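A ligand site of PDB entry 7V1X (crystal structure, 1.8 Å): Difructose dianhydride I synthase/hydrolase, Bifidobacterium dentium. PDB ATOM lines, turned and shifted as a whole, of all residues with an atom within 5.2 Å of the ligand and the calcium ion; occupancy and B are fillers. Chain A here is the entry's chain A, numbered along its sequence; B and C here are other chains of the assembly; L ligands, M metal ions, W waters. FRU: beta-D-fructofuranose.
The side-chain carboxylate (OE2) of Glu 270 lies within hydrogen-bond range of an oxygen (O1) of the ligand, at 2.4 Å. OE2 of Glu 291 is in hydrogen-bond range of O2 of the ligand (2.5 Å). An oxygen (O4) of the ligand lies close to the backbone carbonyl oxygen (O) of Thr 288, at 3.4 Å. OD1 of Asp 292 lies within hydrogen-bond range of O6 of the ligand (2.7 Å). The indole nitrogen (NE1) of Trp 267 lies within hydrogen-bond range of an oxygen (O3) of the ligand, at 2.9 Å. An oxygen (O6) of the ligand sits at hydrogen-bond distance from the backbone NH of Trp 298 (3.0 Å). An oxygen (O3) of the ligand lies within hydrogen-bond range of the backbone carbonyl oxygen (O) of Gly 269, 3.2 Å away.
The side-chain carboxylate (OE2) of Glu 270 lies close to the indole nitrogen (NE1) of Trp 267 (3.5 Å). ND2 of Asn 226 lies within hydrogen-bond range of OE2 of Glu 270 (2.8 Å). The side-chain carboxylate (OE2) of Glu 291 lies within hydrogen-bond range of the backbone NH (N) of Trp 298, at 3.2 Å. The side-chain carboxylate (OE2) of Glu 291 lies within hydrogen-bond range of the backbone NH (N) of Gly 299. O of Glu 291 lies within hydrogen-bond range of N of His 296 (3.0 Å). OG1 of Thr 288 lies within hydrogen-bond range of OD2 of Asp 292 (2.7 Å). OD2 of Asp 292 is in hydrogen-bond range of N of Gly 289. The backbone NH (N) of Tyr 187 of chain B is in hydrogen-bond range of the backbone carbonyl oxygen (O) of Thr 60 of chain B (2.8 Å).
Merely in contact with the ligand: Asn 226 (3.6 Å), Gly 289 (3.8 Å), Ala 297 (3.3 Å), Gly 299 (3.6 Å), Thr 60 of chain B (3.7 Å) and Tyr 187 of chain B (3.4 Å). Hydrophobic or aromatic side chains within 4 Å of the ligand: Trp 267, Ala 297, Trp 298 and Tyr 187 of chain B. Within 4 Å of the ligand: Asn 226, Trp 267, Gly 269, Glu 270, Thr 288, Gly 289, Glu 291, Asp 292, Ala 297, Trp 298, Gly 299, Thr 60 of chain B and Tyr 187 of chain B.
Within 4 Å of the calcium ion: Glu 270, Asn 272, Thr 288, Asn 31 of chain B and Asp 33 of chain B. Along chain A the residues within 4 Å of the calcium ion span positions 270 to 288. The nearest printed residue that does not touch the calcium ion is Gly 289 (4.2 Å).
OD2 of Asp 33 of chain B is bound to the calcium ion, 2.3 Å away. The calcium ion is bound by the backbone carbonyl oxygen (O) of Glu 270. The side-chain amide oxygen (OD1) of Asn 31 of chain B is bound to the calcium ion (2.4 Å). OD1 of Asn 272 is bound to the calcium ion (2.5 Å). Water W3 binds the calcium ion, at 2.5 Å. Water W1 binds the calcium ion, at 2.5 Å. O of Thr 288 is bound to the calcium ion (2.6 Å). The calcium ion has seven donor atoms within binding distance.
Water W1 lies within hydrogen-bond range of the side-chain carboxylate (OE1) of Glu 343, a ring nitrogen (ND1) of His 346 and the side-chain amide nitrogen (ND2) of Asn 272. Water W3 lies within hydrogen-bond range of OE1 of Glu 270 (2.6 Å) and O4 of the ligand (2.8 Å).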
ATOM      1  N   ASN A 226      31.140 -18.096  -4.028  1.00  0.00           N
ATOM      2  CA  ASN A 226      30.722 -19.159  -3.104  1.00  0.00           C
ATOM      3  C   ASN A 226      31.905 -20.086  -2.839  1.00  0.00           C
ATOM      4  O   ASN A 226      31.666 -21.135  -2.245  1.00  0.00           O
ATOM      5  CB  ASN A 226      29.484 -19.921  -3.597  1.00  0.00           C
ATOM      6  CG  ASN A 226      28.231 -19.102  -3.387  1.00  0.00           C
ATOM      7  OD1 ASN A 226      28.182 -18.314  -2.455  1.00  0.00           O
ATOM      8  ND2 ASN A 226      27.255 -19.202  -4.259  1.00  0.00           N
ATOM      9  N   TRP A 267      27.506 -16.557 -10.289  1.00  0.00           N
ATOM     10  CA  TRP A 267      26.264 -15.984  -9.746  1.00  0.00           C
ATOM     11  C   TRP A 267      26.567 -14.615  -9.123  1.00  0.00           C
ATOM     12  O   TRP A 267      27.529 -14.493  -8.360  1.00  0.00           O
ATOM     13  CB  TRP A 267      25.650 -16.978  -8.751  1.00  0.00           C
ATOM     14  CG  TRP A 267      24.513 -16.442  -7.954  1.00  0.00           C
ATOM     15  CD1 TRP A 267      24.452 -16.436  -6.598  1.00  0.00           C
ATOM     16  CD2 TRP A 267      23.287 -15.835  -8.413  1.00  0.00           C
ATOM     17  NE1 TRP A 267      23.260 -15.923  -6.186  1.00  0.00           N
ATOM     18  CE2 TRP A 267      22.546 -15.496  -7.257  1.00  0.00           C
ATOM     19  CE3 TRP A 267      22.769 -15.496  -9.664  1.00  0.00           C
ATOM     20  CZ2 TRP A 267      21.309 -14.902  -7.288  1.00  0.00           C
ATOM     21  CZ3 TRP A 267      21.523 -14.900  -9.706  1.00  0.00           C
ATOM     22  CH2 TRP A 267      20.823 -14.591  -8.543  1.00  0.00           C
ATOM     23  N   GLY A 269      24.523 -12.747  -7.228  1.00  0.00           N
ATOM     24  CA  GLY A 269      23.414 -12.347  -6.333  1.00  0.00           C
ATOM     25  C   GLY A 269      23.507 -12.828  -4.896  1.00  0.00           C
ATOM     26  O   GLY A 269      22.466 -12.878  -4.259  1.00  0.00           O
ATOM     27  N   GLU A 270      24.686 -13.117  -4.364  1.00  0.00           N
ATOM     28  CA  GLU A 270      24.809 -13.589  -2.961  1.00  0.00           C
ATOM     29  C   GLU A 270      24.667 -12.420  -1.980  1.00  0.00           C
ATOM     30  O   GLU A 270      24.528 -12.658  -0.775  1.00  0.00           O
ATOM     31  CB  GLU A 270      26.158 -14.234  -2.713  1.00  0.00           C
ATOM     32  CG  GLU A 270      26.274 -15.588  -3.375  1.00  0.00           C
ATOM     33  CD  GLU A 270      25.335 -16.657  -2.846  1.00  0.00           C
ATOM     34  OE1 GLU A 270      24.932 -16.632  -1.649  1.00  0.00           O
ATOM     35  OE2 GLU A 270      25.027 -17.550  -3.666  1.00  0.00           O
ATOM     36  N   GLY A 271      24.736 -11.194  -2.480  1.00  0.00           N
ATOM     37  CA  GLY A 271      24.764 -10.011  -1.602  1.00  0.00           C
ATOM     38  C   GLY A 271      23.452  -9.758  -0.932  1.00  0.00           C
ATOM     39  O   GLY A 271      22.396  -9.863  -1.551  1.00  0.00           O
ATOM     40  N   ASN A 272      23.503  -9.360   0.338  1.00  0.00           N
ATOM     41  CA  ASN A 272      22.293  -9.071   1.151  1.00  0.00           C
ATOM     42  C   ASN A 272      21.847  -7.638   0.945  1.00  0.00           C
ATOM     43  O   ASN A 272      22.696  -6.740   0.919  1.00  0.00           O
ATOM     44  CB  ASN A 272      22.522  -9.223   2.652  1.00  0.00           C
ATOM     45  CG  ASN A 272      22.949 -10.609   3.074  1.00  0.00           C
ATOM     46  OD1 ASN A 272      22.978 -11.538   2.262  1.00  0.00           O
ATOM     47  ND2 ASN A 272      23.286 -10.763   4.344  1.00  0.00           N
ATOM     48  N   THR A 288      19.271 -11.558   3.074  1.00  0.00           N
ATOM     49  CA  THR A 288      19.938 -12.874   3.015  1.00  0.00           C
ATOM     50  C   THR A 288      20.651 -13.046   1.670  1.00  0.00           C
ATOM     51  O   THR A 288      21.560 -13.876   1.558  1.00  0.00           O
ATOM     52  CB  THR A 288      18.902 -13.950   3.352  1.00  0.00           C
ATOM     53  OG1 THR A 288      17.799 -13.900   2.466  1.00  0.00           O
ATOM     54  CG2 THR A 288      18.381 -13.826   4.775  1.00  0.00           C
ATOM     55  N   GLY A 289      20.208 -12.335   0.650  1.00  0.00           N
ATOM     56  CA  GLY A 289      20.701 -12.509  -0.717  1.00  0.00           C
ATOM     57  C   GLY A 289      19.975 -11.608  -1.674  1.00  0.00           C
ATOM     58  O   GLY A 289      18.951 -10.999  -1.282  1.00  0.00           O
ATOM     59  N   THR A 290      20.473 -11.455  -2.889  1.00  0.00           N
ATOM     60  CA  THR A 290      19.881 -10.445  -3.797  1.00  0.00           C
ATOM     61  C   THR A 290      18.599 -10.999  -4.446  1.00  0.00           C
ATOM     62  O   THR A 290      17.636 -10.251  -4.517  1.00  0.00           O
ATOM     63  CB  THR A 290      20.878  -9.946  -4.830  1.00  0.00           C
ATOM     64  OG1 THR A 290      22.119  -9.649  -4.184  1.00  0.00           O
ATOM     65  CG2 THR A 290      20.358  -8.691  -5.515  1.00  0.00           C
ATOM     66  N   GLU A 291      18.595 -12.247  -4.936  1.00  0.00           N
ATOM     67  CA  GLU A 291      17.345 -12.850  -5.459  1.00  0.00           C
ATOM     68  C   GLU A 291      16.393 -12.942  -4.286  1.00  0.00           C
ATOM     69  O   GLU A 291      15.210 -12.763  -4.479  1.00  0.00           O
ATOM     70  CB  GLU A 291      17.535 -14.182  -6.202  1.00  0.00           C
ATOM     71  CG  GLU A 291      17.632 -15.428  -5.320  1.00  0.00           C
ATOM     72  CD  GLU A 291      19.038 -15.736  -4.831  1.00  0.00           C
ATOM     73  OE1 GLU A 291      19.672 -14.805  -4.249  1.00  0.00           O
ATOM     74  OE2 GLU A 291      19.526 -16.898  -5.060  1.00  0.00           O
ATOM     75  N   ASP A 292      16.912 -13.167  -3.076  1.00  0.00           N
ATOM     76  CA  ASP A 292      15.994 -13.256  -1.914  1.00  0.00           C
ATOM     77  C   ASP A 292      15.287 -11.931  -1.732  1.00  0.00           C
ATOM     78  O   ASP A 292      14.068 -11.954  -1.436  1.00  0.00           O
ATOM     79  CB  ASP A 292      16.737 -13.632  -0.651  1.00  0.00           C
ATOM     80  CG  ASP A 292      17.588 -14.879  -0.797  1.00  0.00           C
ATOM     81  OD1 ASP A 292      17.473 -15.573  -1.883  1.00  0.00           O
ATOM     82  OD2 ASP A 292      18.383 -15.109   0.137  1.00  0.00           O
ATOM     83  N   HIS A 296      12.683 -14.163  -5.113  1.00  0.00           N
ATOM     84  CA  HIS A 296      12.981 -15.446  -5.821  1.00  0.00           C
ATOM     85  C   HIS A 296      13.879 -16.266  -4.891  1.00  0.00           C
ATOM     86  O   HIS A 296      14.043 -15.880  -3.715  1.00  0.00           O
ATOM     87  CB  HIS A 296      13.505 -15.178  -7.233  1.00  0.00           C
ATOM     88  CG  HIS A 296      12.443 -14.714  -8.167  1.00  0.00           C
ATOM     89  ND1 HIS A 296      12.633 -14.732  -9.545  1.00  0.00           N
ATOM     90  CD2 HIS A 296      11.186 -14.260  -7.955  1.00  0.00           C
ATOM     91  CE1 HIS A 296      11.538 -14.269 -10.126  1.00  0.00           C
ATOM     92  NE2 HIS A 296      10.629 -13.975  -9.180  1.00  0.00           N
ATOM     93  N   ALA A 297      14.407 -17.391  -5.369  1.00  0.00           N
ATOM     94  CA  ALA A 297      15.323 -18.220  -4.561  1.00  0.00           C
ATOM     95  C   ALA A 297      16.161 -19.088  -5.468  1.00  0.00           C
ATOM     96  O   ALA A 297      15.577 -19.605  -6.451  1.00  0.00           O
ATOM     97  CB  ALA A 297      14.517 -19.032  -3.576  1.00  0.00           C
ATOM     98  N   TRP A 298      17.428 -19.334  -5.084  1.00  0.00           N
ATOM     99  CA  TRP A 298      18.333 -20.260  -5.792  1.00  0.00           C
ATOM    100  C   TRP A 298      18.500 -19.716  -7.213  1.00  0.00           C
ATOM    101  O   TRP A 298      18.322 -20.451  -8.183  1.00  0.00           O
ATOM    102  CB  TRP A 298      17.757 -21.692  -5.769  1.00  0.00           C
ATOM    103  CG  TRP A 298      17.291 -22.108  -4.413  1.00  0.00           C
ATOM    104  CD1 TRP A 298      16.001 -22.189  -3.997  1.00  0.00           C
ATOM    105  CD2 TRP A 298      18.100 -22.408  -3.255  1.00  0.00           C
ATOM    106  NE1 TRP A 298      15.939 -22.551  -2.689  1.00  0.00           N
ATOM    107  CE2 TRP A 298      17.213 -22.691  -2.199  1.00  0.00           C
ATOM    108  CE3 TRP A 298      19.479 -22.488  -3.021  1.00  0.00           C
ATOM    109  CZ2 TRP A 298      17.656 -23.070  -0.935  1.00  0.00           C
ATOM    110  CZ3 TRP A 298      19.921 -22.848  -1.773  1.00  0.00           C
ATOM    111  CH2 TRP A 298      19.011 -23.139  -0.745  1.00  0.00           C
ATOM    112  N   GLY A 299      18.794 -18.428  -7.302  1.00  0.00           N
ATOM    113  CA  GLY A 299      18.780 -17.750  -8.597  1.00  0.00           C
ATOM    114  C   GLY A 299      17.510 -16.932  -8.831  1.00  0.00           C
ATOM    115  O   GLY A 299      16.550 -16.995  -8.058  1.00  0.00           O
ATOM    116  N   GLU A 343      24.711  -5.613  -0.852  1.00  0.00           N
ATOM    117  CA  GLU A 343      26.129  -6.000  -1.036  1.00  0.00           C
ATOM    118  C   GLU A 343      26.263  -6.420  -2.513  1.00  0.00           C
ATOM    119  O   GLU A 343      25.375  -7.164  -2.991  1.00  0.00           O
ATOM    120  CB  GLU A 343      26.484  -7.194  -0.176  1.00  0.00           C
ATOM    121  CG  GLU A 343      26.211  -7.049   1.306  1.00  0.00           C
ATOM    122  CD  GLU A 343      26.584  -8.359   1.989  1.00  0.00           C
ATOM    123  OE1 GLU A 343      25.826  -9.316   1.800  1.00  0.00           O
ATOM    124  OE2 GLU A 343      27.692  -8.422   2.630  1.00  0.00           O
ATOM    125  N   HIS A 346      28.589 -11.296  -2.200  1.00  0.00           N
ATOM    126  CA  HIS A 346      28.806 -11.461  -0.768  1.00  0.00           C
ATOM    127  C   HIS A 346      29.922 -10.494  -0.325  1.00  0.00           C
ATOM    128  O   HIS A 346      31.026 -10.554  -0.874  1.00  0.00           O
ATOM    129  CB  HIS A 346      29.227 -12.893  -0.396  1.00  0.00           C
ATOM    130  CG  HIS A 346      29.577 -12.914   1.046  1.00  0.00           C
ATOM    131  ND1 HIS A 346      28.653 -12.485   1.999  1.00  0.00           N
ATOM    132  CD2 HIS A 346      30.733 -13.159   1.692  1.00  0.00           C
ATOM    133  CE1 HIS A 346      29.231 -12.493   3.182  1.00  0.00           C
ATOM    134  NE2 HIS A 346      30.511 -12.907   3.030  1.00  0.00           N
ATOM    135  N   ASN B  31      28.365 -15.495   4.764  1.00  0.00           N
ATOM    136  CA  ASN B  31      27.398 -15.784   3.683  1.00  0.00           C
ATOM    137  C   ASN B  31      26.651 -17.081   3.976  1.00  0.00           C
ATOM    138  O   ASN B  31      26.198 -17.691   3.014  1.00  0.00           O
ATOM    139  CB  ASN B  31      28.059 -15.860   2.305  1.00  0.00           C
ATOM    140  CG  ASN B  31      27.061 -15.696   1.189  1.00  0.00           C
ATOM    141  OD1 ASN B  31      26.058 -14.994   1.338  1.00  0.00           O
ATOM    142  ND2 ASN B  31      27.286 -16.398   0.093  1.00  0.00           N
ATOM    143  N   ASP B  33      23.386 -17.089   5.236  1.00  0.00           N
ATOM    144  CA  ASP B  33      22.201 -16.256   5.616  1.00  0.00           C
ATOM    145  C   ASP B  33      20.952 -17.121   5.719  1.00  0.00           C
ATOM    146  O   ASP B  33      19.854 -16.635   5.422  1.00  0.00           O
ATOM    147  CB  ASP B  33      22.034 -15.141   4.594  1.00  0.00           C
ATOM    148  CG  ASP B  33      23.286 -14.306   4.551  1.00  0.00           C
ATOM    149  OD1 ASP B  33      23.520 -13.521   5.516  1.00  0.00           O
ATOM    150  OD2 ASP B  33      24.016 -14.419   3.573  1.00  0.00           O
ATOM    151  N   TRP B  58       8.869 -13.776   3.220  1.00  0.00           N
ATOM    152  CA  TRP B  58       9.511 -14.529   2.134  1.00  0.00           C
ATOM    153  C   TRP B  58      10.346 -15.631   2.809  1.00  0.00           C
ATOM    154  O   TRP B  58      11.024 -15.358   3.821  1.00  0.00           O
ATOM    155  CB  TRP B  58      10.393 -13.616   1.316  1.00  0.00           C
ATOM    156  CG  TRP B  58      11.326 -14.410   0.469  1.00  0.00           C
ATOM    157  CD1 TRP B  58      11.056 -14.830  -0.808  1.00  0.00           C
ATOM    158  CD2 TRP B  58      12.628 -14.924   0.819  1.00  0.00           C
ATOM    159  NE1 TRP B  58      12.115 -15.548  -1.286  1.00  0.00           N
ATOM    160  CE2 TRP B  58      13.092 -15.619  -0.328  1.00  0.00           C
ATOM    161  CE3 TRP B  58      13.482 -14.805   1.918  1.00  0.00           C
ATOM    162  CZ2 TRP B  58      14.357 -16.216  -0.379  1.00  0.00           C
ATOM    163  CZ3 TRP B  58      14.708 -15.431   1.896  1.00  0.00           C
ATOM    164  CH2 TRP B  58      15.141 -16.120   0.759  1.00  0.00           C
ATOM    165  N   THR B  60      12.704 -19.515   1.681  1.00  0.00           N
ATOM    166  CA  THR B  60      13.013 -20.680   0.838  1.00  0.00           C
ATOM    167  C   THR B  60      13.675 -21.707   1.727  1.00  0.00           C
ATOM    168  O   THR B  60      14.010 -21.384   2.893  1.00  0.00           O
ATOM    169  CB  THR B  60      13.824 -20.309  -0.404  1.00  0.00           C
ATOM    170  OG1 THR B  60      13.686 -21.479  -1.219  1.00  0.00           O
ATOM    171  CG2 THR B  60      15.275 -19.962  -0.119  1.00  0.00           C
ATOM    172  N   ALA B  81      28.622 -23.038  -1.395  1.00  0.00           N
ATOM    173  CA  ALA B  81      27.163 -22.847  -1.530  1.00  0.00           C
ATOM    174  C   ALA B  81      26.454 -23.791  -0.566  1.00  0.00           C
ATOM    175  O   ALA B  81      26.936 -24.848  -0.180  1.00  0.00           O
ATOM    176  CB  ALA B  81      26.728 -23.056  -2.961  1.00  0.00           C
ATOM    177  N   PRO B  82      25.230 -23.459  -0.115  1.00  0.00           N
ATOM    178  CA  PRO B  82      24.610 -24.266   0.925  1.00  0.00           C
ATOM    179  C   PRO B  82      24.042 -25.626   0.483  1.00  0.00           C
ATOM    180  O   PRO B  82      23.847 -26.529   1.348  1.00  0.00           O
ATOM    181  CB  PRO B  82      23.442 -23.407   1.390  1.00  0.00           C
ATOM    182  CG  PRO B  82      23.184 -22.506   0.262  1.00  0.00           C
ATOM    183  CD  PRO B  82      24.502 -22.219  -0.395  1.00  0.00           C
ATOM    184  N   TYR B 187      15.773 -20.222   4.794  1.00  0.00           N
ATOM    185  CA  TYR B 187      16.016 -18.782   4.584  1.00  0.00           C
ATOM    186  C   TYR B 187      14.687 -18.089   4.870  1.00  0.00           C
ATOM    187  O   TYR B 187      13.644 -18.588   4.426  1.00  0.00           O
ATOM    188  CB  TYR B 187      16.386 -18.497   3.131  1.00  0.00           C
ATOM    189  CG  TYR B 187      17.790 -18.842   2.699  1.00  0.00           C
ATOM    190  CD1 TYR B 187      18.151 -20.103   2.262  1.00  0.00           C
ATOM    191  CD2 TYR B 187      18.757 -17.860   2.646  1.00  0.00           C
ATOM    192  CE1 TYR B 187      19.446 -20.372   1.834  1.00  0.00           C
ATOM    193  CE2 TYR B 187      20.048 -18.114   2.225  1.00  0.00           C
ATOM    194  CZ  TYR B 187      20.381 -19.367   1.767  1.00  0.00           C
ATOM    195  OH  TYR B 187      21.686 -19.584   1.376  1.00  0.00           O
ATOM    196  N   ALA C  89      28.653 -21.534  -9.683  1.00  0.00           N
ATOM    197  CA  ALA C  89      28.018 -20.832  -8.564  1.00  0.00           C
ATOM    198  C   ALA C  89      28.025 -21.697  -7.292  1.00  0.00           C
ATOM    199  O   ALA C  89      27.707 -21.131  -6.230  1.00  0.00           O
ATOM    200  CB  ALA C  89      26.632 -20.410  -8.938  1.00  0.00           C
HETATM  201  C1  FRU L   1      22.421 -19.796  -3.072  1.00  0.00           C
HETATM  202  C2  FRU L   1      21.509 -18.575  -3.496  1.00  0.00           C
HETATM  203  C3  FRU L   1      21.821 -17.259  -2.756  1.00  0.00           C
HETATM  204  C4  FRU L   1      20.560 -17.112  -1.842  1.00  0.00           C
HETATM  205  C5  FRU L   1      20.056 -18.549  -1.665  1.00  0.00           C
HETATM  206  C6  FRU L   1      18.600 -18.759  -1.302  1.00  0.00           C
HETATM  207  O1  FRU L   1      23.775 -19.581  -3.391  1.00  0.00           O
HETATM  208  O2  FRU L   1      21.502 -18.411  -4.936  1.00  0.00           O
HETATM  209  O3  FRU L   1      22.082 -16.004  -3.518  1.00  0.00           O
HETATM  210  O4  FRU L   1      20.729 -16.341  -0.591  1.00  0.00           O
HETATM  211  O5  FRU L   1      20.261 -19.041  -2.949  1.00  0.00           O
HETATM  212  O6  FRU L   1      17.722 -18.193  -2.290  1.00  0.00           O
HETATM  213 CA    CA M   1      24.119 -13.553   1.428  1.00  0.00          CA
HETATM  214  O   HOH W   1      25.886 -12.012   2.392  1.00  0.00           O
HETATM  215  O   HOH W   2      21.984 -20.494  -6.422  1.00  0.00           O
HETATM  216  O   HOH W   3      23.343 -15.585   0.188  1.00  0.00           O
